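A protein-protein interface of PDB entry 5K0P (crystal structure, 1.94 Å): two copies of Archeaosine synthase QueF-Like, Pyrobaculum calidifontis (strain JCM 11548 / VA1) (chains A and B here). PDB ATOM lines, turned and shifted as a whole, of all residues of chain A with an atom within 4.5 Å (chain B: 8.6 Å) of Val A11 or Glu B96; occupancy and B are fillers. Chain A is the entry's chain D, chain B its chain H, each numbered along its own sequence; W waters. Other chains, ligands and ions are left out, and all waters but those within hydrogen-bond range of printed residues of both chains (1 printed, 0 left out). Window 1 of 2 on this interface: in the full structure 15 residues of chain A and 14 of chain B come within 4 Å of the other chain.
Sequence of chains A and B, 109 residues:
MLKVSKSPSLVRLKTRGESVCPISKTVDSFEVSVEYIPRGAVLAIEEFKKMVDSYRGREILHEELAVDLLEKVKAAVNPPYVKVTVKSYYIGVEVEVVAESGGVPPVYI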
ATOM      1  N   PRO A   8      13.739  10.148  10.569  1.00  0.00           N
ATOM      2  CA  PRO A   8      15.096   9.756  10.362  1.00  0.00           C
ATOM      3  C   PRO A   8      15.183   8.631   9.313  1.00  0.00           C
ATOM      4  O   PRO A   8      14.180   7.866   9.142  1.00  0.00           O
ATOM      5  CB  PRO A   8      15.528   9.232  11.731  1.00  0.00           C
ATOM      6  CG  PRO A   8      14.581   9.812  12.716  1.00  0.00           C
ATOM      7  CD  PRO A   8      13.311   9.921  11.945  1.00  0.00           C
ATOM      8  N   LEU A  10      17.593   6.262   9.588  1.00  0.00           N
ATOM      9  CA  LEU A  10      18.000   5.078  10.395  1.00  0.00           C
ATOM     10  C   LEU A  10      18.121   5.495  11.828  1.00  0.00           C
ATOM     11  O   LEU A  10      18.580   6.619  12.116  1.00  0.00           O
ATOM     12  CB  LEU A  10      19.395   4.596  10.002  1.00  0.00           C
ATOM     13  CG  LEU A  10      19.863   3.308  10.750  1.00  0.00           C
ATOM     14  CD1 LEU A  10      19.117   2.146  10.264  1.00  0.00           C
ATOM     15  CD2 LEU A  10      21.324   3.074  10.510  1.00  0.00           C
ATOM     16  N   VAL A  11      17.724   4.581  12.715  1.00  0.00           N
ATOM     17  CA  VAL A  11      17.953   4.661  14.148  1.00  0.00           C
ATOM     18  C   VAL A  11      18.662   3.418  14.680  1.00  0.00           C
ATOM     19  O   VAL A  11      18.284   2.274  14.348  1.00  0.00           O
ATOM     20  CB  VAL A  11      16.619   4.786  14.844  1.00  0.00           C
ATOM     21  CG1 VAL A  11      16.784   4.886  16.356  1.00  0.00           C
ATOM     22  CG2 VAL A  11      15.855   5.986  14.287  1.00  0.00           C
ATOM     23  N   ARG A  12      19.621   3.657  15.566  1.00  0.00           N
ATOM     24  CA  ARG A  12      20.254   2.610  16.358  1.00  0.00           C
ATOM     25  C   ARG A  12      20.068   2.860  17.839  1.00  0.00           C
ATOM     26  O   ARG A  12      20.284   3.968  18.331  1.00  0.00           O
ATOM     27  CB  ARG A  12      21.756   2.486  16.115  1.00  0.00           C
ATOM     28  CG  ARG A  12      22.142   2.028  14.735  1.00  0.00           C
ATOM     29  CD  ARG A  12      23.641   1.649  14.735  1.00  0.00           C
ATOM     30  NE  ARG A  12      24.229   2.670  13.919  1.00  0.00           N
ATOM     31  CZ  ARG A  12      24.286   2.630  12.609  1.00  0.00           C
ATOM     32  NH1 ARG A  12      23.908   1.528  11.947  1.00  0.00           N
ATOM     33  NH2 ARG A  12      24.764   3.690  11.969  1.00  0.00           N
ATOM     34  N   LEU A  13      19.735   1.787  18.528  1.00  0.00           N
ATOM     35  CA  LEU A  13      19.543   1.829  19.966  1.00  0.00           C
ATOM     36  C   LEU A  13      20.374   0.731  20.586  1.00  0.00           C
ATOM     37  O   LEU A  13      20.507  -0.345  19.999  1.00  0.00           O
ATOM     38  CB  LEU A  13      18.104   1.603  20.282  1.00  0.00           C
ATOM     39  CG  LEU A  13      17.087   2.490  19.601  1.00  0.00           C
ATOM     40  CD1 LEU A  13      15.751   1.797  19.724  1.00  0.00           C
ATOM     41  CD2 LEU A  13      17.050   3.886  20.199  1.00  0.00           C
ATOM     42  N   VAL A  34      19.421  -2.546  18.588  1.00  0.00           N
ATOM     43  CA  VAL A  34      18.405  -2.602  17.535  1.00  0.00           C
ATOM     44  C   VAL A  34      18.670  -1.532  16.534  1.00  0.00           C
ATOM     45  O   VAL A  34      18.966  -0.414  16.871  1.00  0.00           O
ATOM     46  CB  VAL A  34      17.053  -2.413  18.127  1.00  0.00           C
ATOM     47  CG1 VAL A  34      15.943  -2.424  17.075  1.00  0.00           C
ATOM     48  CG2 VAL A  34      16.831  -3.492  19.171  1.00  0.00           C
ATOM     49  N   GLU A  35      18.591  -1.862  15.277  1.00  0.00           N
ATOM     50  CA  GLU A  35      18.639  -0.855  14.305  1.00  0.00           C
ATOM     51  C   GLU A  35      17.513  -1.097  13.390  1.00  0.00           C
ATOM     52  O   GLU A  35      17.155  -2.264  13.108  1.00  0.00           O
ATOM     53  CB  GLU A  35      19.921  -0.804  13.578  1.00  0.00           C
ATOM     54  CG  GLU A  35      20.324  -1.955  12.749  1.00  0.00           C
ATOM     55  CD  GLU A  35      21.716  -1.787  12.195  1.00  0.00           C
ATOM     56  OE1 GLU A  35      22.634  -1.371  12.947  1.00  0.00           O
ATOM     57  OE2 GLU A  35      21.855  -2.085  10.998  1.00  0.00           O
ATOM     58  N   TYR A  36      16.933  -0.004  12.939  1.00  0.00           N
ATOM     59  CA  TYR A  36      15.755  -0.092  12.095  1.00  0.00           C
ATOM     60  C   TYR A  36      15.569   1.165  11.222  1.00  0.00           C
ATOM     61  O   TYR A  36      16.105   2.248  11.515  1.00  0.00           O
ATOM     62  CB  TYR A  36      14.483  -0.319  12.957  1.00  0.00           C
ATOM     63  CG  TYR A  36      13.985   0.908  13.722  1.00  0.00           C
ATOM     64  CD1 TYR A  36      14.510   1.233  14.978  1.00  0.00           C
ATOM     65  CD2 TYR A  36      12.993   1.731  13.191  1.00  0.00           C
ATOM     66  CE1 TYR A  36      14.065   2.327  15.694  1.00  0.00           C
ATOM     67  CE2 TYR A  36      12.518   2.837  13.907  1.00  0.00           C
ATOM     68  CZ  TYR A  36      13.079   3.114  15.170  1.00  0.00           C
ATOM     69  OH  TYR A  36      12.738   4.216  15.870  1.00  0.00           O
ATOM     70  N   PRO A  38      12.947   3.804   9.960  1.00  0.00           N
ATOM     71  CA  PRO A  38      11.580   4.206  10.231  1.00  0.00           C
ATOM     72  C   PRO A  38      10.769   4.253   8.965  1.00  0.00           C
ATOM     73  O   PRO A  38      11.320   4.532   7.876  1.00  0.00           O
ATOM     74  CB  PRO A  38      11.720   5.607  10.807  1.00  0.00           C
ATOM     75  CG  PRO A  38      13.080   5.589  11.476  1.00  0.00           C
ATOM     76  CD  PRO A  38      13.920   4.724  10.586  1.00  0.00           C
ATOM     77  N   GLU B  31      26.364  14.462  20.583  1.00  0.00           N
ATOM     78  CA  GLU B  31      27.432  14.559  19.585  1.00  0.00           C
ATOM     79  C   GLU B  31      26.784  14.482  18.222  1.00  0.00           C
ATOM     80  O   GLU B  31      25.912  13.689  18.000  1.00  0.00           O
ATOM     81  CB  GLU B  31      28.415  13.415  19.759  1.00  0.00           C
ATOM     82  CG  GLU B  31      29.481  13.379  18.642  1.00  0.00           C
ATOM     83  CD  GLU B  31      30.191  12.037  18.562  1.00  0.00           C
ATOM     84  OE1 GLU B  31      29.704  11.169  17.756  1.00  0.00           O
ATOM     85  OE2 GLU B  31      31.232  11.895  19.273  1.00  0.00           O
ATOM     86  N   SER B  33      27.504  14.492  13.901  1.00  0.00           N
ATOM     87  CA  SER B  33      28.404  14.343  12.789  1.00  0.00           C
ATOM     88  C   SER B  33      27.619  14.648  11.536  1.00  0.00           C
ATOM     89  O   SER B  33      26.478  14.154  11.333  1.00  0.00           O
ATOM     90  CB  SER B  33      28.980  12.896  12.688  1.00  0.00           C
ATOM     91  OG  SER B  33      29.423  12.456  14.006  1.00  0.00           O
ATOM     92  N   HIS B  62      15.974  14.502  19.731  1.00  0.00           N
ATOM     93  CA  HIS B  62      17.163  14.288  18.847  1.00  0.00           C
ATOM     94  C   HIS B  62      16.824  13.698  17.512  1.00  0.00           C
ATOM     95  O   HIS B  62      17.438  14.073  16.502  1.00  0.00           O
ATOM     96  CB  HIS B  62      18.273  13.538  19.571  1.00  0.00           C
ATOM     97  CG  HIS B  62      18.861  14.352  20.678  1.00  0.00           C
ATOM     98  ND1 HIS B  62      19.669  13.835  21.666  1.00  0.00           N
ATOM     99  CD2 HIS B  62      18.686  15.667  20.984  1.00  0.00           C
ATOM    100  CE1 HIS B  62      20.002  14.801  22.516  1.00  0.00           C
ATOM    101  NE2 HIS B  62      19.416  15.930  22.118  1.00  0.00           N
ATOM    102  N   GLU B  63      15.806  12.842  17.485  1.00  0.00           N
ATOM    103  CA  GLU B  63      15.170  12.339  16.218  1.00  0.00           C
ATOM    104  C   GLU B  63      14.750  13.468  15.266  1.00  0.00           C
ATOM    105  O   GLU B  63      14.861  13.313  14.059  1.00  0.00           O
ATOM    106  CB  GLU B  63      13.966  11.379  16.545  1.00  0.00           C
ATOM    107  CG  GLU B  63      12.682  12.079  17.001  1.00  0.00           C
ATOM    108  CD  GLU B  63      11.521  11.195  17.417  1.00  0.00           C
ATOM    109  OE1 GLU B  63      10.369  11.392  16.910  1.00  0.00           O
ATOM    110  OE2 GLU B  63      11.709  10.350  18.289  1.00  0.00           O
ATOM    111  N   ALA B  66      18.119  15.877  14.104  1.00  0.00           N
ATOM    112  CA  ALA B  66      18.970  15.416  13.013  1.00  0.00           C
ATOM    113  C   ALA B  66      18.413  15.838  11.669  1.00  0.00           C
ATOM    114  O   ALA B  66      19.154  16.203  10.726  1.00  0.00           O
ATOM    115  CB  ALA B  66      19.117  13.916  13.101  1.00  0.00           C
ATOM    116  N   VAL B  84      23.430  13.383   8.427  1.00  0.00           N
ATOM    117  CA  VAL B  84      23.562  13.950   9.769  1.00  0.00           C
ATOM    118  C   VAL B  84      23.353  12.796  10.760  1.00  0.00           C
ATOM    119  O   VAL B  84      22.366  12.084  10.636  1.00  0.00           O
ATOM    120  CB  VAL B  84      22.500  15.039   9.988  1.00  0.00           C
ATOM    121  CG1 VAL B  84      22.577  15.562  11.437  1.00  0.00           C
ATOM    122  CG2 VAL B  84      22.779  16.191   9.048  1.00  0.00           C
ATOM    123  N   THR B  85      24.277  12.607  11.714  1.00  0.00           N
ATOM    124  CA  THR B  85      24.138  11.580  12.726  1.00  0.00           C
ATOM    125  C   THR B  85      24.160  12.248  14.096  1.00  0.00           C
ATOM    126  O   THR B  85      25.026  12.999  14.366  1.00  0.00           O
ATOM    127  CB  THR B  85      25.272  10.548  12.605  1.00  0.00           C
ATOM    128  OG1 THR B  85      25.209   9.965  11.296  1.00  0.00           O
ATOM    129  CG2 THR B  85      25.146   9.440  13.699  1.00  0.00           C
ATOM    130  N   VAL B  86      23.138  12.027  14.896  1.00  0.00           N
ATOM    131  CA  VAL B  86      23.124  12.591  16.258  1.00  0.00           C
ATOM    132  C   VAL B  86      23.152  11.420  17.205  1.00  0.00           C
ATOM    133  O   VAL B  86      22.222  10.561  17.178  1.00  0.00           O
ATOM    134  CB  VAL B  86      21.839  13.385  16.534  1.00  0.00           C
ATOM    135  CG1 VAL B  86      21.761  13.879  17.968  1.00  0.00           C
ATOM    136  CG2 VAL B  86      21.719  14.564  15.590  1.00  0.00           C
ATOM    137  N   LYS B  87      24.108  11.476  18.135  1.00  0.00           N
ATOM    138  CA  LYS B  87      24.247  10.453  19.183  1.00  0.00           C
ATOM    139  C   LYS B  87      24.016  11.038  20.547  1.00  0.00           C
ATOM    140  O   LYS B  87      24.618  12.026  20.892  1.00  0.00           O
ATOM    141  CB  LYS B  87      25.635   9.767  19.197  1.00  0.00           C
ATOM    142  CG  LYS B  87      25.939   9.111  17.864  1.00  0.00           C
ATOM    143  CD  LYS B  87      27.205   8.169  17.796  1.00  0.00           C
ATOM    144  CE  LYS B  87      27.823   8.187  16.372  1.00  0.00           C
ATOM    145  NZ  LYS B  87      29.203   7.584  16.231  1.00  0.00           N
ATOM    146  N   SER B  88      23.245  10.355  21.372  1.00  0.00           N
ATOM    147  CA  SER B  88      23.075  10.770  22.698  1.00  0.00           C
ATOM    148  C   SER B  88      22.707   9.555  23.601  1.00  0.00           C
ATOM    149  O   SER B  88      22.655   8.425  23.180  1.00  0.00           O
ATOM    150  CB  SER B  88      21.995  11.875  22.726  1.00  0.00           C
ATOM    151  OG  SER B  88      20.879  11.502  21.947  1.00  0.00           O
ATOM    152  N   TYR B  89      22.465   9.817  24.868  1.00  0.00           N
ATOM    153  CA  TYR B  89      22.321   8.770  25.862  1.00  0.00           C
ATOM    154  C   TYR B  89      21.199   9.170  26.771  1.00  0.00           C
ATOM    155  O   TYR B  89      21.165  10.256  27.347  1.00  0.00           O
ATOM    156  CB  TYR B  89      23.670   8.593  26.555  1.00  0.00           C
ATOM    157  CG  TYR B  89      23.771   7.466  27.537  1.00  0.00           C
ATOM    158  CD1 TYR B  89      23.717   6.145  27.082  1.00  0.00           C
ATOM    159  CD2 TYR B  89      24.032   7.698  28.940  1.00  0.00           C
ATOM    160  CE1 TYR B  89      23.836   5.062  27.967  1.00  0.00           C
ATOM    161  CE2 TYR B  89      24.193   6.617  29.835  1.00  0.00           C
ATOM    162  CZ  TYR B  89      24.092   5.292  29.333  1.00  0.00           C
ATOM    163  OH  TYR B  89      24.246   4.142  30.139  1.00  0.00           O
ATOM    164  N   VAL B  93      19.909   4.250  27.490  1.00  0.00           N
ATOM    165  CA  VAL B  93      19.942   3.818  26.081  1.00  0.00           C
ATOM    166  C   VAL B  93      20.900   4.705  25.300  1.00  0.00           C
ATOM    167  O   VAL B  93      20.772   5.937  25.366  1.00  0.00           O
ATOM    168  CB  VAL B  93      18.531   3.849  25.435  1.00  0.00           C
ATOM    169  CG1 VAL B  93      18.586   3.335  24.004  1.00  0.00           C
ATOM    170  CG2 VAL B  93      17.574   2.998  26.238  1.00  0.00           C
ATOM    171  N   GLU B  94      21.872   4.122  24.617  1.00  0.00           N
ATOM    172  CA  GLU B  94      22.635   4.817  23.588  1.00  0.00           C
ATOM    173  C   GLU B  94      21.802   4.931  22.309  1.00  0.00           C
ATOM    174  O   GLU B  94      21.381   3.911  21.752  1.00  0.00           O
ATOM    175  CB  GLU B  94      23.926   4.119  23.223  1.00  0.00           C
ATOM    176  CG  GLU B  94      24.868   3.971  24.405  1.00  0.00           C
ATOM    177  CD  GLU B  94      26.041   3.123  24.048  1.00  0.00           C
ATOM    178  OE1 GLU B  94      26.734   3.417  23.010  1.00  0.00           O
ATOM    179  OE2 GLU B  94      26.189   2.140  24.788  1.00  0.00           O
ATOM    180  N   VAL B  95      21.590   6.159  21.862  1.00  0.00           N
ATOM    181  CA  VAL B  95      20.741   6.431  20.725  1.00  0.00           C
ATOM    182  C   VAL B  95      21.603   7.080  19.602  1.00  0.00           C
ATOM    183  O   VAL B  95      22.377   7.996  19.877  1.00  0.00           O
ATOM    184  CB  VAL B  95      19.623   7.407  21.103  1.00  0.00           C
ATOM    185  CG1 VAL B  95      18.665   7.556  19.893  1.00  0.00           C
ATOM    186  CG2 VAL B  95      18.868   6.968  22.364  1.00  0.00           C
ATOM    187  N   GLU B  96      21.477   6.580  18.370  1.00  0.00           N
ATOM    188  CA  GLU B  96      21.945   7.287  17.202  1.00  0.00           C
ATOM    189  C   GLU B  96      20.814   7.413  16.212  1.00  0.00           C
ATOM    190  O   GLU B  96      20.208   6.404  15.808  1.00  0.00           O
ATOM    191  CB  GLU B  96      23.026   6.590  16.398  1.00  0.00           C
ATOM    192  CG  GLU B  96      24.102   6.000  17.161  1.00  0.00           C
ATOM    193  CD  GLU B  96      25.156   5.451  16.241  1.00  0.00           C
ATOM    194  OE1 GLU B  96      24.958   5.253  15.020  1.00  0.00           O
ATOM    195  OE2 GLU B  96      26.196   5.240  16.830  1.00  0.00           O
ATOM    196  N   VAL B  97      20.633   8.643  15.736  1.00  0.00           N
ATOM    197  CA  VAL B  97      19.649   8.937  14.792  1.00  0.00           C
ATOM    198  C   VAL B  97      20.380   9.451  13.557  1.00  0.00           C
ATOM    199  O   VAL B  97      21.186  10.336  13.653  1.00  0.00           O
ATOM    200  CB  VAL B  97      18.718  10.006  15.364  1.00  0.00           C
ATOM    201  CG1 VAL B  97      17.690  10.356  14.357  1.00  0.00           C
ATOM    202  CG2 VAL B  97      17.960   9.448  16.541  1.00  0.00           C
ATOM    203  N   VAL B  98      20.057   8.935  12.380  1.00  0.00           N
ATOM    204  CA  VAL B  98      20.701   9.331  11.183  1.00  0.00           C
ATOM    205  C   VAL B  98      19.616   9.944  10.260  1.00  0.00           C
ATOM    206  O   VAL B  98      18.518   9.368  10.076  1.00  0.00           O
ATOM    207  CB  VAL B  98      21.297   8.079  10.477  1.00  0.00           C
ATOM    208  CG1 VAL B  98      21.967   8.431   9.148  1.00  0.00           C
ATOM    209  CG2 VAL B  98      22.337   7.380  11.325  1.00  0.00           C
ATOM    210  N   ALA B  99      19.937  11.078   9.646  1.00  0.00           N
ATOM    211  CA  ALA B  99      19.073  11.686   8.621  1.00  0.00           C
ATOM    212  C   ALA B  99      19.883  11.885   7.373  1.00  0.00           C
ATOM    213  O   ALA B  99      20.984  12.297   7.429  1.00  0.00           O
ATOM    214  CB  ALA B  99      18.519  13.006   9.076  1.00  0.00           C
HETATM  215  O   HOH W   1      23.087   3.308  19.572  1.00  0.00           O
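N of Val B98 is in hydrogen-bond range of O of Leu A10, at 2.8 Å.
The side-chain carboxylate of Glu B96 is in salt-bridge range of the guanidinium group of Arg A12 (2.9 Å).
The guanidinium group of Arg A12 lies within salt-bridge range of the side-chain carboxylate of Glu A35 (3.3 Å).
The backbone NH (N) of Tyr A36 lies within hydrogen-bond range of the backbone carbonyl oxygen (O) of Val A11 (3.0 Å).
The backbone NH (N) of Val B86 is in hydrogen-bond range of the backbone carbonyl oxygen (O) of Val B97, 2.9 Å away.
NZ of Lys B87 is in salt-bridge range of OE2 of Glu B96 (3.9 Å).
The backbone carbonyl oxygen (O) of Ser B88 is in hydrogen-bond range of the backbone NH (N) of Val B95 (2.8 Å).
The backbone NH (N) of Val A34 lies within hydrogen-bond range of the backbone carbonyl oxygen (O) of Leu A13.
O of Glu B63 touches CG of Pro A8 (3.8 Å).
Val B97 touches Pro A8.
Pro A8 touches Val B98 (CB to O, 3.4 Å).
C of Val B97 touches O of Leu A10, 3.7 Å away.
Val A11 touches Glu B96 (CA to O, 3.3 Å).
Arg A12 touches Glu B94.
Val B95 touches Arg A12 (CA to O, 3.5 Å).
Leu A13 touches Glu B94 (CA to O, 3.3 Å).
Of the printed residues of chain B, Arg A12 touches Glu B94, Val B95 and Glu B96.
Printed residues of chain A within 4 Å of Val B95: Arg A12.
Of the printed residues of chain A, Glu B96 touches Val A11 (3.3 Å) and Arg A12 (2.8 Å).
Printed residues of chain A within 4 Å of Val B97: Pro A8 and Leu A10.
Of the printed residues of chain A, Val B98 touches Pro A8 and Leu A10.
Ala B99 touches none of the printed residues of chain A.
The nearest residue of chain B that does not touch Val A11 is Val B97 (4.6 Å).
The nearest residue of chain A that does not touch Glu B96 is Leu A10 (4.04 Å).
Of the 9 printed residues of chain A, 5 touch a printed residue of chain B.
Hydrophobic or aromatic side chains of chain A within 4 Å of the printed part of chain B: Pro A8, Leu A10 and Val A11.
Hydrophobic or aromatic side chains of chain B that line the printed part of chain A: Val B97 and Val B98.
Among the printed residues, 10 pairs touch across the chains.
Among the printed residues, Asp or Glu carboxylates within 4 Å of a Lys or Arg side-chain nitrogen of the other chain: Arg A12 with Glu B96 (2.9 Å).
No position is printed for both chains.
Of the 10 pairs that touch across the chains among the printed residues, none has its exchanged pair printed and touching as well.
Water W1 lies within hydrogen-bond range of the backbone carbonyl oxygen (O) of Glu B94 (2.8 Å) and the backbone carbonyl oxygen (O) of Arg A12 (3.1 Å).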
